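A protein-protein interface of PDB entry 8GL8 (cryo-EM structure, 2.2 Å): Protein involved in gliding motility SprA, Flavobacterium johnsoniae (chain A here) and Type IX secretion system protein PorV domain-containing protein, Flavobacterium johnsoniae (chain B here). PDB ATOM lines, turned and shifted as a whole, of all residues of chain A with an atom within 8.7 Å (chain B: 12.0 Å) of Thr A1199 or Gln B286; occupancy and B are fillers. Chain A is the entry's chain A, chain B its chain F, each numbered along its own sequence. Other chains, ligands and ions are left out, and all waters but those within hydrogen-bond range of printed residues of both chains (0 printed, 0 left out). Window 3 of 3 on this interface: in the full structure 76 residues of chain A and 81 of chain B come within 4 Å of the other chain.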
ATOM      1  N   ARG A 936      -6.230  -2.182   7.209  1.00  0.00           N
ATOM      2  CA  ARG A 936      -5.790  -1.178   8.166  1.00  0.00           C
ATOM      3  C   ARG A 936      -5.211  -1.826   9.418  1.00  0.00           C
ATOM      4  O   ARG A 936      -5.585  -2.935   9.807  1.00  0.00           O
ATOM      5  CB  ARG A 936      -6.948  -0.254   8.542  1.00  0.00           C
ATOM      6  CG  ARG A 936      -8.060  -0.923   9.329  1.00  0.00           C
ATOM      7  CD  ARG A 936      -9.208   0.039   9.577  1.00  0.00           C
ATOM      8  NE  ARG A 936     -10.295  -0.583  10.323  1.00  0.00           N
ATOM      9  CZ  ARG A 936     -10.348  -0.663  11.645  1.00  0.00           C
ATOM     10  NH1 ARG A 936      -9.385  -0.170  12.406  1.00  0.00           N
ATOM     11  NH2 ARG A 936     -11.391  -1.252  12.219  1.00  0.00           N
ATOM     12  N   GLU A 942      -8.861  -0.379  20.284  1.00  0.00           N
ATOM     13  CA  GLU A 942     -10.121  -0.514  19.562  1.00  0.00           C
ATOM     14  C   GLU A 942     -10.824  -1.817  19.923  1.00  0.00           C
ATOM     15  O   GLU A 942     -12.020  -1.823  20.232  1.00  0.00           O
ATOM     16  CB  GLU A 942      -9.880  -0.435  18.054  1.00  0.00           C
ATOM     17  CG  GLU A 942     -11.077  -0.864  17.219  1.00  0.00           C
ATOM     18  CD  GLU A 942     -10.779  -0.887  15.734  1.00  0.00           C
ATOM     19  OE1 GLU A 942      -9.984  -0.045  15.270  1.00  0.00           O
ATOM     20  OE2 GLU A 942     -11.345  -1.747  15.027  1.00  0.00           O
ATOM     21  N   VAL A1016     -19.376  -4.190   6.893  1.00  0.00           N
ATOM     22  CA  VAL A1016     -19.627  -2.919   7.557  1.00  0.00           C
ATOM     23  C   VAL A1016     -18.629  -1.844   7.142  1.00  0.00           C
ATOM     24  O   VAL A1016     -19.021  -0.706   6.860  1.00  0.00           O
ATOM     25  CB  VAL A1016     -19.631  -3.092   9.092  1.00  0.00           C
ATOM     26  CG1 VAL A1016     -19.506  -1.748   9.795  1.00  0.00           C
ATOM     27  CG2 VAL A1016     -20.892  -3.815   9.536  1.00  0.00           C
ATOM     28  N   ARG A1196     -19.050  -5.566  19.321  1.00  0.00           N
ATOM     29  CA  ARG A1196     -18.528  -4.247  19.652  1.00  0.00           C
ATOM     30  C   ARG A1196     -18.515  -3.399  18.389  1.00  0.00           C
ATOM     31  O   ARG A1196     -17.899  -3.778  17.388  1.00  0.00           O
ATOM     32  CB  ARG A1196     -17.126  -4.351  20.252  1.00  0.00           C
ATOM     33  CG  ARG A1196     -16.404  -3.022  20.380  1.00  0.00           C
ATOM     34  CD  ARG A1196     -15.150  -3.151  21.229  1.00  0.00           C
ATOM     35  NE  ARG A1196     -15.453  -3.422  22.629  1.00  0.00           N
ATOM     36  CZ  ARG A1196     -15.889  -2.515  23.492  1.00  0.00           C
ATOM     37  NH1 ARG A1196     -16.089  -1.258  23.132  1.00  0.00           N
ATOM     38  NH2 ARG A1196     -16.123  -2.875  24.750  1.00  0.00           N
ATOM     39  N   GLU A1197     -19.188  -2.256  18.434  1.00  0.00           N
ATOM     40  CA  GLU A1197     -19.259  -1.348  17.299  1.00  0.00           C
ATOM     41  C   GLU A1197     -18.227  -0.242  17.465  1.00  0.00           C
ATOM     42  O   GLU A1197     -18.096   0.335  18.549  1.00  0.00           O
ATOM     43  CB  GLU A1197     -20.659  -0.751  17.162  1.00  0.00           C
ATOM     44  CG  GLU A1197     -21.775  -1.773  17.250  1.00  0.00           C
ATOM     45  CD  GLU A1197     -22.439  -2.027  15.914  1.00  0.00           C
ATOM     46  OE1 GLU A1197     -22.006  -1.423  14.909  1.00  0.00           O
ATOM     47  OE2 GLU A1197     -23.395  -2.828  15.866  1.00  0.00           O
ATOM     48  N   VAL A1198     -17.495   0.045  16.393  1.00  0.00           N
ATOM     49  CA  VAL A1198     -16.493   1.102  16.365  1.00  0.00           C
ATOM     50  C   VAL A1198     -16.992   2.155  15.386  1.00  0.00           C
ATOM     51  O   VAL A1198     -17.213   1.856  14.206  1.00  0.00           O
ATOM     52  CB  VAL A1198     -15.114   0.564  15.954  1.00  0.00           C
ATOM     53  CG1 VAL A1198     -14.029   1.555  16.308  1.00  0.00           C
ATOM     54  CG2 VAL A1198     -14.851  -0.779  16.618  1.00  0.00           C
ATOM     55  N   THR A1199     -17.164   3.382  15.872  1.00  0.00           N
ATOM     56  CA  THR A1199     -17.913   4.389  15.128  1.00  0.00           C
ATOM     57  C   THR A1199     -17.029   5.224  14.206  1.00  0.00           C
ATOM     58  O   THR A1199     -17.311   5.335  13.010  1.00  0.00           O
ATOM     59  CB  THR A1199     -18.673   5.294  16.103  1.00  0.00           C
ATOM     60  OG1 THR A1199     -19.840   4.609  16.574  1.00  0.00           O
ATOM     61  CG2 THR A1199     -19.107   6.581  15.417  1.00  0.00           C
ATOM     62  N   ASN A1200     -15.962   5.822  14.731  1.00  0.00           N
ATOM     63  CA  ASN A1200     -15.116   6.722  13.944  1.00  0.00           C
ATOM     64  C   ASN A1200     -13.671   6.249  14.050  1.00  0.00           C
ATOM     65  O   ASN A1200     -12.926   6.688  14.929  1.00  0.00           O
ATOM     66  CB  ASN A1200     -15.276   8.166  14.409  1.00  0.00           C
ATOM     67  CG  ASN A1200     -16.648   8.728  14.098  1.00  0.00           C
ATOM     68  OD1 ASN A1200     -17.167   8.556  12.995  1.00  0.00           O
ATOM     69  ND2 ASN A1200     -17.246   9.401  15.073  1.00  0.00           N
ATOM     70  N   VAL A1201     -13.280   5.357  13.146  1.00  0.00           N
ATOM     71  CA  VAL A1201     -11.906   4.874  13.091  1.00  0.00           C
ATOM     72  C   VAL A1201     -11.076   5.871  12.295  1.00  0.00           C
ATOM     73  O   VAL A1201     -11.386   6.164  11.136  1.00  0.00           O
ATOM     74  CB  VAL A1201     -11.831   3.476  12.461  1.00  0.00           C
ATOM     75  CG1 VAL A1201     -10.411   2.945  12.529  1.00  0.00           C
ATOM     76  CG2 VAL A1201     -12.797   2.529  13.140  1.00  0.00           C
ATOM     77  N   ASP A1202     -10.021   6.392  12.911  1.00  0.00           N
ATOM     78  CA  ASP A1202      -9.095   7.246  12.186  1.00  0.00           C
ATOM     79  C   ASP A1202      -8.328   6.424  11.161  1.00  0.00           C
ATOM     80  O   ASP A1202      -7.881   5.309  11.443  1.00  0.00           O
ATOM     81  CB  ASP A1202      -8.127   7.928  13.149  1.00  0.00           C
ATOM     82  CG  ASP A1202      -8.700   9.195  13.745  1.00  0.00           C
ATOM     83  OD1 ASP A1202      -8.612   9.362  14.978  1.00  0.00           O
ATOM     84  OD2 ASP A1202      -9.245  10.021  12.981  1.00  0.00           O
ATOM     85  N   GLY A1207      -9.637   9.904   6.353  1.00  0.00           N
ATOM     86  CA  GLY A1207     -11.052   9.635   6.482  1.00  0.00           C
ATOM     87  C   GLY A1207     -11.382   8.846   7.734  1.00  0.00           C
ATOM     88  O   GLY A1207     -10.528   8.563   8.578  1.00  0.00           O
ATOM     89  N   THR A1208     -12.657   8.489   7.849  1.00  0.00           N
ATOM     90  CA  THR A1208     -13.156   7.691   8.956  1.00  0.00           C
ATOM     91  C   THR A1208     -14.003   6.550   8.413  1.00  0.00           C
ATOM     92  O   THR A1208     -14.541   6.623   7.305  1.00  0.00           O
ATOM     93  CB  THR A1208     -13.983   8.530   9.943  1.00  0.00           C
ATOM     94  OG1 THR A1208     -14.882   9.377   9.217  1.00  0.00           O
ATOM     95  CG2 THR A1208     -13.073   9.385  10.808  1.00  0.00           C
ATOM     96  N   THR A1209     -14.115   5.489   9.205  1.00  0.00           N
ATOM     97  CA  THR A1209     -14.879   4.323   8.792  1.00  0.00           C
ATOM     98  C   THR A1209     -15.555   3.700  10.003  1.00  0.00           C
ATOM     99  O   THR A1209     -15.142   3.901  11.147  1.00  0.00           O
ATOM    100  CB  THR A1209     -13.992   3.290   8.079  1.00  0.00           C
ATOM    101  OG1 THR A1209     -14.815   2.342   7.388  1.00  0.00           O
ATOM    102  CG2 THR A1209     -13.101   2.556   9.072  1.00  0.00           C
ATOM    103  N   ASN A1210     -16.620   2.955   9.730  1.00  0.00           N
ATOM    104  CA  ASN A1210     -17.285   2.132  10.725  1.00  0.00           C
ATOM    105  C   ASN A1210     -16.625   0.760  10.787  1.00  0.00           C
ATOM    106  O   ASN A1210     -15.979   0.312   9.838  1.00  0.00           O
ATOM    107  CB  ASN A1210     -18.772   1.976  10.395  1.00  0.00           C
ATOM    108  CG  ASN A1210     -19.606   3.130  10.902  1.00  0.00           C
ATOM    109  OD1 ASN A1210     -19.154   3.924  11.720  1.00  0.00           O
ATOM    110  ND2 ASN A1210     -20.838   3.227  10.415  1.00  0.00           N
ATOM    111  N   ALA A1211     -16.794   0.093  11.925  1.00  0.00           N
ATOM    112  CA  ALA A1211     -16.291  -1.263  12.076  1.00  0.00           C
ATOM    113  C   ALA A1211     -17.165  -2.007  13.072  1.00  0.00           C
ATOM    114  O   ALA A1211     -17.820  -1.405  13.925  1.00  0.00           O
ATOM    115  CB  ALA A1211     -14.826  -1.278  12.527  1.00  0.00           C
ATOM    116  N   ARG A1212     -17.158  -3.330  12.962  1.00  0.00           N
ATOM    117  CA  ARG A1212     -17.917  -4.181  13.867  1.00  0.00           C
ATOM    118  C   ARG A1212     -17.087  -5.412  14.184  1.00  0.00           C
ATOM    119  O   ARG A1212     -16.706  -6.157  13.277  1.00  0.00           O
ATOM    120  CB  ARG A1212     -19.265  -4.577  13.258  1.00  0.00           C
ATOM    121  CG  ARG A1212     -20.413  -4.579  14.243  1.00  0.00           C
ATOM    122  CD  ARG A1212     -21.749  -4.523  13.529  1.00  0.00           C
ATOM    123  NE  ARG A1212     -22.165  -5.835  13.052  1.00  0.00           N
ATOM    124  CZ  ARG A1212     -23.162  -6.539  13.568  1.00  0.00           C
ATOM    125  NH1 ARG A1212     -23.877  -6.083  14.583  1.00  0.00           N
ATOM    126  NH2 ARG A1212     -23.453  -7.727  13.050  1.00  0.00           N
ATOM    127  N   TRP A1213     -16.805  -5.621  15.465  1.00  0.00           N
ATOM    128  CA  TRP A1213     -16.102  -6.801  15.938  1.00  0.00           C
ATOM    129  C   TRP A1213     -17.113  -7.760  16.548  1.00  0.00           C
ATOM    130  O   TRP A1213     -17.933  -7.360  17.377  1.00  0.00           O
ATOM    131  CB  TRP A1213     -15.038  -6.426  16.969  1.00  0.00           C
ATOM    132  CG  TRP A1213     -13.818  -5.796  16.381  1.00  0.00           C
ATOM    133  CD1 TRP A1213     -13.551  -4.464  16.284  1.00  0.00           C
ATOM    134  CD2 TRP A1213     -12.694  -6.474  15.808  1.00  0.00           C
ATOM    135  NE1 TRP A1213     -12.331  -4.268  15.688  1.00  0.00           N
ATOM    136  CE2 TRP A1213     -11.784  -5.487  15.385  1.00  0.00           C
ATOM    137  CE3 TRP A1213     -12.370  -7.818  15.613  1.00  0.00           C
ATOM    138  CZ2 TRP A1213     -10.572  -5.803  14.779  1.00  0.00           C
ATOM    139  CZ3 TRP A1213     -11.169  -8.128  15.010  1.00  0.00           C
ATOM    140  CH2 TRP A1213     -10.283  -7.126  14.601  1.00  0.00           C
ATOM    141  N   THR A1297     -19.827  -4.498  26.206  1.00  0.00           N
ATOM    142  CA  THR A1297     -20.898  -4.167  25.273  1.00  0.00           C
ATOM    143  C   THR A1297     -21.765  -5.384  24.966  1.00  0.00           C
ATOM    144  O   THR A1297     -22.317  -5.498  23.871  1.00  0.00           O
ATOM    145  CB  THR A1297     -20.337  -3.576  23.978  1.00  0.00           C
ATOM    146  OG1 THR A1297     -19.625  -4.586  23.254  1.00  0.00           O
ATOM    147  CG2 THR A1297     -19.403  -2.415  24.270  1.00  0.00           C
ATOM    148  N   PRO B 262     -10.250  11.607  29.376  1.00  0.00           N
ATOM    149  CA  PRO B 262     -11.637  11.586  29.852  1.00  0.00           C
ATOM    150  C   PRO B 262     -11.925  10.349  30.686  1.00  0.00           C
ATOM    151  O   PRO B 262     -11.328   9.287  30.497  1.00  0.00           O
ATOM    152  CB  PRO B 262     -12.457  11.589  28.557  1.00  0.00           C
ATOM    153  CG  PRO B 262     -11.548  10.979  27.546  1.00  0.00           C
ATOM    154  CD  PRO B 262     -10.166  11.438  27.915  1.00  0.00           C
ATOM    155  N   GLY B 263     -12.864  10.497  31.618  1.00  0.00           N
ATOM    156  CA  GLY B 263     -13.174   9.447  32.560  1.00  0.00           C
ATOM    157  C   GLY B 263     -14.460   8.710  32.248  1.00  0.00           C
ATOM    158  O   GLY B 263     -14.680   8.238  31.128  1.00  0.00           O
ATOM    159  N   PRO B 264     -15.334   8.580  33.256  1.00  0.00           N
ATOM    160  CA  PRO B 264     -16.586   7.834  33.067  1.00  0.00           C
ATOM    161  C   PRO B 264     -17.475   8.429  31.985  1.00  0.00           C
ATOM    162  O   PRO B 264     -18.163   7.699  31.265  1.00  0.00           O
ATOM    163  CB  PRO B 264     -17.257   7.915  34.447  1.00  0.00           C
ATOM    164  CG  PRO B 264     -16.162   8.301  35.397  1.00  0.00           C
ATOM    165  CD  PRO B 264     -15.228   9.153  34.606  1.00  0.00           C
ATOM    166  N   GLY B 265     -17.466   9.752  31.866  1.00  0.00           N
ATOM    167  CA  GLY B 265     -18.258  10.425  30.858  1.00  0.00           C
ATOM    168  C   GLY B 265     -18.268  11.929  31.033  1.00  0.00           C
ATOM    169  O   GLY B 265     -18.410  12.429  32.152  1.00  0.00           O
ATOM    170  N   THR B 266     -18.123  12.660  29.932  1.00  0.00           N
ATOM    171  CA  THR B 266     -18.106  14.115  29.985  1.00  0.00           C
ATOM    172  C   THR B 266     -19.069  14.695  28.955  1.00  0.00           C
ATOM    173  O   THR B 266     -18.633  15.189  27.908  1.00  0.00           O
ATOM    174  CB  THR B 266     -16.693  14.649  29.749  1.00  0.00           C
ATOM    175  OG1 THR B 266     -15.738  13.750  30.326  1.00  0.00           O
ATOM    176  CG2 THR B 266     -16.530  16.023  30.379  1.00  0.00           C
ATOM    177  N   PRO B 267     -20.387  14.652  29.211  1.00  0.00           N
ATOM    178  CA  PRO B 267     -21.385  15.201  28.285  1.00  0.00           C
ATOM    179  C   PRO B 267     -21.283  16.716  28.147  1.00  0.00           C
ATOM    180  O   PRO B 267     -22.314  17.373  27.996  1.00  0.00           O
ATOM    181  CB  PRO B 267     -22.722  14.803  28.926  1.00  0.00           C
ATOM    182  CG  PRO B 267     -22.385  13.725  29.909  1.00  0.00           C
ATOM    183  CD  PRO B 267     -21.015  14.050  30.397  1.00  0.00           C
ATOM    184  N   SER B 283     -26.212   5.608  22.849  1.00  0.00           N
ATOM    185  CA  SER B 283     -24.812   5.954  22.632  1.00  0.00           C
ATOM    186  C   SER B 283     -24.041   5.940  23.946  1.00  0.00           C
ATOM    187  O   SER B 283     -23.803   6.988  24.548  1.00  0.00           O
ATOM    188  CB  SER B 283     -24.696   7.327  21.965  1.00  0.00           C
ATOM    189  OG  SER B 283     -25.222   8.345  22.797  1.00  0.00           O
ATOM    190  N   GLN B 284     -23.649   4.745  24.388  1.00  0.00           N
ATOM    191  CA  GLN B 284     -22.928   4.593  25.648  1.00  0.00           C
ATOM    192  C   GLN B 284     -21.417   4.626  25.436  1.00  0.00           C
ATOM    193  O   GLN B 284     -20.724   5.486  25.989  1.00  0.00           O
ATOM    194  CB  GLN B 284     -23.349   3.289  26.336  1.00  0.00           C
ATOM    195  CG  GLN B 284     -24.302   3.484  27.502  1.00  0.00           C
ATOM    196  CD  GLN B 284     -25.662   3.994  27.064  1.00  0.00           C
ATOM    197  OE1 GLN B 284     -26.328   3.382  26.229  1.00  0.00           O
ATOM    198  NE2 GLN B 284     -26.080   5.121  27.627  1.00  0.00           N
ATOM    199  N   SER B 285     -20.894   3.694  24.637  1.00  0.00           N
ATOM    200  CA  SER B 285     -19.473   3.691  24.318  1.00  0.00           C
ATOM    201  C   SER B 285     -19.115   4.707  23.244  1.00  0.00           C
ATOM    202  O   SER B 285     -17.934   5.042  23.095  1.00  0.00           O
ATOM    203  CB  SER B 285     -19.035   2.292  23.876  1.00  0.00           C
ATOM    204  OG  SER B 285     -19.997   1.699  23.021  1.00  0.00           O
ATOM    205  N   GLN B 286     -20.104   5.203  22.496  1.00  0.00           N
ATOM    206  CA  GLN B 286     -19.835   6.219  21.483  1.00  0.00           C
ATOM    207  C   GLN B 286     -19.318   7.504  22.115  1.00  0.00           C
ATOM    208  O   GLN B 286     -18.397   8.139  21.586  1.00  0.00           O
ATOM    209  CB  GLN B 286     -21.097   6.494  20.667  1.00  0.00           C
ATOM    210  CG  GLN B 286     -21.098   5.867  19.285  1.00  0.00           C
ATOM    211  CD  GLN B 286     -22.348   6.199  18.496  1.00  0.00           C
ATOM    212  OE1 GLN B 286     -23.208   6.949  18.958  1.00  0.00           O
ATOM    213  NE2 GLN B 286     -22.458   5.639  17.297  1.00  0.00           N
ATOM    214  N   ALA B 287     -19.906   7.909  23.244  1.00  0.00           N
ATOM    215  CA  ALA B 287     -19.455   9.121  23.920  1.00  0.00           C
ATOM    216  C   ALA B 287     -18.021   8.976  24.411  1.00  0.00           C
ATOM    217  O   ALA B 287     -17.210   9.898  24.263  1.00  0.00           O
ATOM    218  CB  ALA B 287     -20.391   9.454  25.080  1.00  0.00           C
ATOM    219  N   ASP B 288     -17.689   7.823  24.997  1.00  0.00           N
ATOM    220  CA  ASP B 288     -16.322   7.587  25.449  1.00  0.00           C
ATOM    221  C   ASP B 288     -15.349   7.577  24.278  1.00  0.00           C
ATOM    222  O   ASP B 288     -14.243   8.125  24.373  1.00  0.00           O
ATOM    223  CB  ASP B 288     -16.244   6.270  26.221  1.00  0.00           C
ATOM    224  CG  ASP B 288     -16.857   6.367  27.603  1.00  0.00           C
ATOM    225  OD1 ASP B 288     -16.923   7.489  28.148  1.00  0.00           O
ATOM    226  OD2 ASP B 288     -17.272   5.322  28.144  1.00  0.00           O
ATOM    227  N   GLU B 289     -15.743   6.955  23.164  1.00  0.00           N
ATOM    228  CA  GLU B 289     -14.884   6.933  21.985  1.00  0.00           C
ATOM    229  C   GLU B 289     -14.637   8.339  21.454  1.00  0.00           C
ATOM    230  O   GLU B 289     -13.502   8.690  21.116  1.00  0.00           O
ATOM    231  CB  GLU B 289     -15.501   6.054  20.900  1.00  0.00           C
ATOM    232  CG  GLU B 289     -14.509   5.599  19.849  1.00  0.00           C
ATOM    233  CD  GLU B 289     -15.096   4.589  18.887  1.00  0.00           C
ATOM    234  OE1 GLU B 289     -14.371   4.167  17.965  1.00  0.00           O
ATOM    235  OE2 GLU B 289     -16.277   4.217  19.050  1.00  0.00           O
ATOM    236  N   ALA B 290     -15.687   9.160  21.375  1.00  0.00           N
ATOM    237  CA  ALA B 290     -15.521  10.529  20.896  1.00  0.00           C
ATOM    238  C   ALA B 290     -14.660  11.350  21.848  1.00  0.00           C
ATOM    239  O   ALA B 290     -13.830  12.158  21.407  1.00  0.00           O
ATOM    240  CB  ALA B 290     -16.886  11.187  20.702  1.00  0.00           C
ATOM    241  N   ASN B 291     -14.844  11.163  23.158  1.00  0.00           N
ATOM    242  CA  ASN B 291     -14.033  11.885  24.130  1.00  0.00           C
ATOM    243  C   ASN B 291     -12.562  11.507  24.011  1.00  0.00           C
ATOM    244  O   ASN B 291     -11.685  12.379  24.044  1.00  0.00           O
ATOM    245  CB  ASN B 291     -14.547  11.616  25.543  1.00  0.00           C
ATOM    246  CG  ASN B 291     -15.763  12.450  25.888  1.00  0.00           C
ATOM    247  OD1 ASN B 291     -15.945  13.549  25.364  1.00  0.00           O
ATOM    248  ND2 ASN B 291     -16.606  11.931  26.773  1.00  0.00           N
ATOM    249  N   TYR B 292     -12.270  10.213  23.861  1.00  0.00           N
ATOM    250  CA  TYR B 292     -10.883   9.795  23.683  1.00  0.00           C
ATOM    251  C   TYR B 292     -10.319  10.299  22.362  1.00  0.00           C
ATOM    252  O   TYR B 292      -9.137  10.652  22.279  1.00  0.00           O
ATOM    253  CB  TYR B 292     -10.769   8.274  23.770  1.00  0.00           C
ATOM    254  CG  TYR B 292      -9.383   7.806  24.149  1.00  0.00           C
ATOM    255  CD1 TYR B 292      -8.426   7.548  23.177  1.00  0.00           C
ATOM    256  CD2 TYR B 292      -9.028   7.634  25.480  1.00  0.00           C
ATOM    257  CE1 TYR B 292      -7.156   7.126  23.519  1.00  0.00           C
ATOM    258  CE2 TYR B 292      -7.762   7.213  25.831  1.00  0.00           C
ATOM    259  CZ  TYR B 292      -6.830   6.960  24.847  1.00  0.00           C
ATOM    260  OH  TYR B 292      -5.567   6.540  25.195  1.00  0.00           O
ATOM    261  N   LYS B 293     -11.147  10.332  21.315  1.00  0.00           N
ATOM    262  CA  LYS B 293     -10.710  10.860  20.028  1.00  0.00           C
ATOM    263  C   LYS B 293     -10.311  12.325  20.145  1.00  0.00           C
ATOM    264  O   LYS B 293      -9.279  12.745  19.611  1.00  0.00           O
ATOM    265  CB  LYS B 293     -11.826  10.682  18.998  1.00  0.00           C
ATOM    266  CG  LYS B 293     -11.679  11.527  17.742  1.00  0.00           C
ATOM    267  CD  LYS B 293     -10.995  10.760  16.630  1.00  0.00           C
ATOM    268  CE  LYS B 293     -10.991  11.558  15.335  1.00  0.00           C
ATOM    269  NZ  LYS B 293      -9.743  12.350  15.162  1.00  0.00           N
ATOM    270  N   LYS B 294     -11.119  13.120  20.849  1.00  0.00           N
ATOM    271  CA  LYS B 294     -10.793  14.536  20.993  1.00  0.00           C
ATOM    272  C   LYS B 294      -9.629  14.751  21.955  1.00  0.00           C
ATOM    273  O   LYS B 294      -8.887  15.730  21.816  1.00  0.00           O
ATOM    274  CB  LYS B 294     -12.025  15.324  21.445  1.00  0.00           C
ATOM    275  CG  LYS B 294     -12.260  15.347  22.944  1.00  0.00           C
ATOM    276  CD  LYS B 294     -13.624  15.928  23.278  1.00  0.00           C
ATOM    277  CE  LYS B 294     -13.815  17.285  22.620  1.00  0.00           C
ATOM    278  NZ  LYS B 294     -13.287  18.390  23.465  1.00  0.00           N
ATOM    279  N   TYR B 295      -9.446  13.854  22.929  1.00  0.00           N
ATOM    280  CA  TYR B 295      -8.324  13.987  23.851  1.00  0.00           C
ATOM    281  C   TYR B 295      -7.002  13.652  23.173  1.00  0.00           C
ATOM    282  O   TYR B 295      -6.005  14.357  23.359  1.00  0.00           O
ATOM    283  CB  TYR B 295      -8.544  13.093  25.072  1.00  0.00           C
ATOM    284  CG  TYR B 295      -7.271  12.693  25.783  1.00  0.00           C
ATOM    285  CD1 TYR B 295      -6.613  13.579  26.625  1.00  0.00           C
ATOM    286  CD2 TYR B 295      -6.727  11.425  25.616  1.00  0.00           C
ATOM    287  CE1 TYR B 295      -5.451  13.216  27.277  1.00  0.00           C
ATOM    288  CE2 TYR B 295      -5.566  11.054  26.262  1.00  0.00           C
ATOM    289  CZ  TYR B 295      -4.932  11.953  27.092  1.00  0.00           C
ATOM    290  OH  TYR B 295      -3.775  11.585  27.738  1.00  0.00           O
ATOM    291  N   LYS B 296      -6.972  12.576  22.383  1.00  0.00           N
ATOM    292  CA  LYS B 296      -5.731  12.153  21.746  1.00  0.00           C
ATOM    293  C   LYS B 296      -5.319  13.075  20.606  1.00  0.00           C
ATOM    294  O   LYS B 296      -4.144  13.076  20.224  1.00  0.00           O
ATOM    295  CB  LYS B 296      -5.866  10.713  21.246  1.00  0.00           C
ATOM    296  CG  LYS B 296      -6.172  10.579  19.763  1.00  0.00           C
ATOM    297  CD  LYS B 296      -6.538   9.148  19.408  1.00  0.00           C
ATOM    298  CE  LYS B 296      -6.392   8.892  17.918  1.00  0.00           C
ATOM    299  NZ  LYS B 296      -7.692   9.018  17.203  1.00  0.00           N
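The side-chain amide nitrogen (NE2) of Gln B286 lies within hydrogen-bond range of the side-chain hydroxyl (OG1) of Thr A1199, 2.9 Å away.
The backbone NH (N) of Thr A1199 lies within hydrogen-bond range of the side-chain carboxylate (OE2) of Glu B289 (3.4 Å).
OD1 of Asp A1202 is in salt-bridge range of NZ of Lys B293, at 3.2 Å.
The side-chain amino group of Lys B296 lies within salt-bridge range of the side-chain carboxylate of Asp A1202, 2.4 Å away.
The backbone NH (N) of Val A1198 is in hydrogen-bond range of the backbone carbonyl oxygen (O) of Ala A1211 (2.9 Å).
O of Thr A1199 sits close to OD1 of Asn A1210, 2.7 Å away.
Val A1198 touches Glu B289.
Asn A1200 touches Glu B289 (N to OE1, 3.97 Å).
Of chain B, only Gln B286 (2.9 Å) and Glu B289 (3.4 Å) come within 4 Å of Thr A1199.
Of chain B, only Glu B289 (3.97 Å) comes within 4 Å of Asn A1200.
No residue of chain B comes within 4 Å of Val A1201.
Printed residues of chain B within 4 Å of Asp A1202: Lys B293 (3.2 Å) and Lys B296 (2.4 Å).
No residue of chain B comes within 4 Å of Thr A1208.
No residue of chain B comes within 4 Å of Asn A1210.
No residue of chain B comes within 4 Å of Ala A1211.
Gln B284 touches none of the printed residues of chain A.
No residue of chain A comes within 4 Å of Ser B285.
Printed residues of chain A within 4 Å of Glu B289: Val A1198 (3.1 Å), Thr A1199 (3.4 Å) and Asn A1200 (3.97 Å).
Printed residues of chain A within 4 Å of Lys B293: Asp A1202.
Of the printed residues of chain A, Lys B296 touches Asp A1202.
The nearest residue of chain A that does not touch Gln B286 is Glu A1197 (6.3 Å).
Of the 18 printed residues of chain A, 4 touch a printed residue of chain B.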
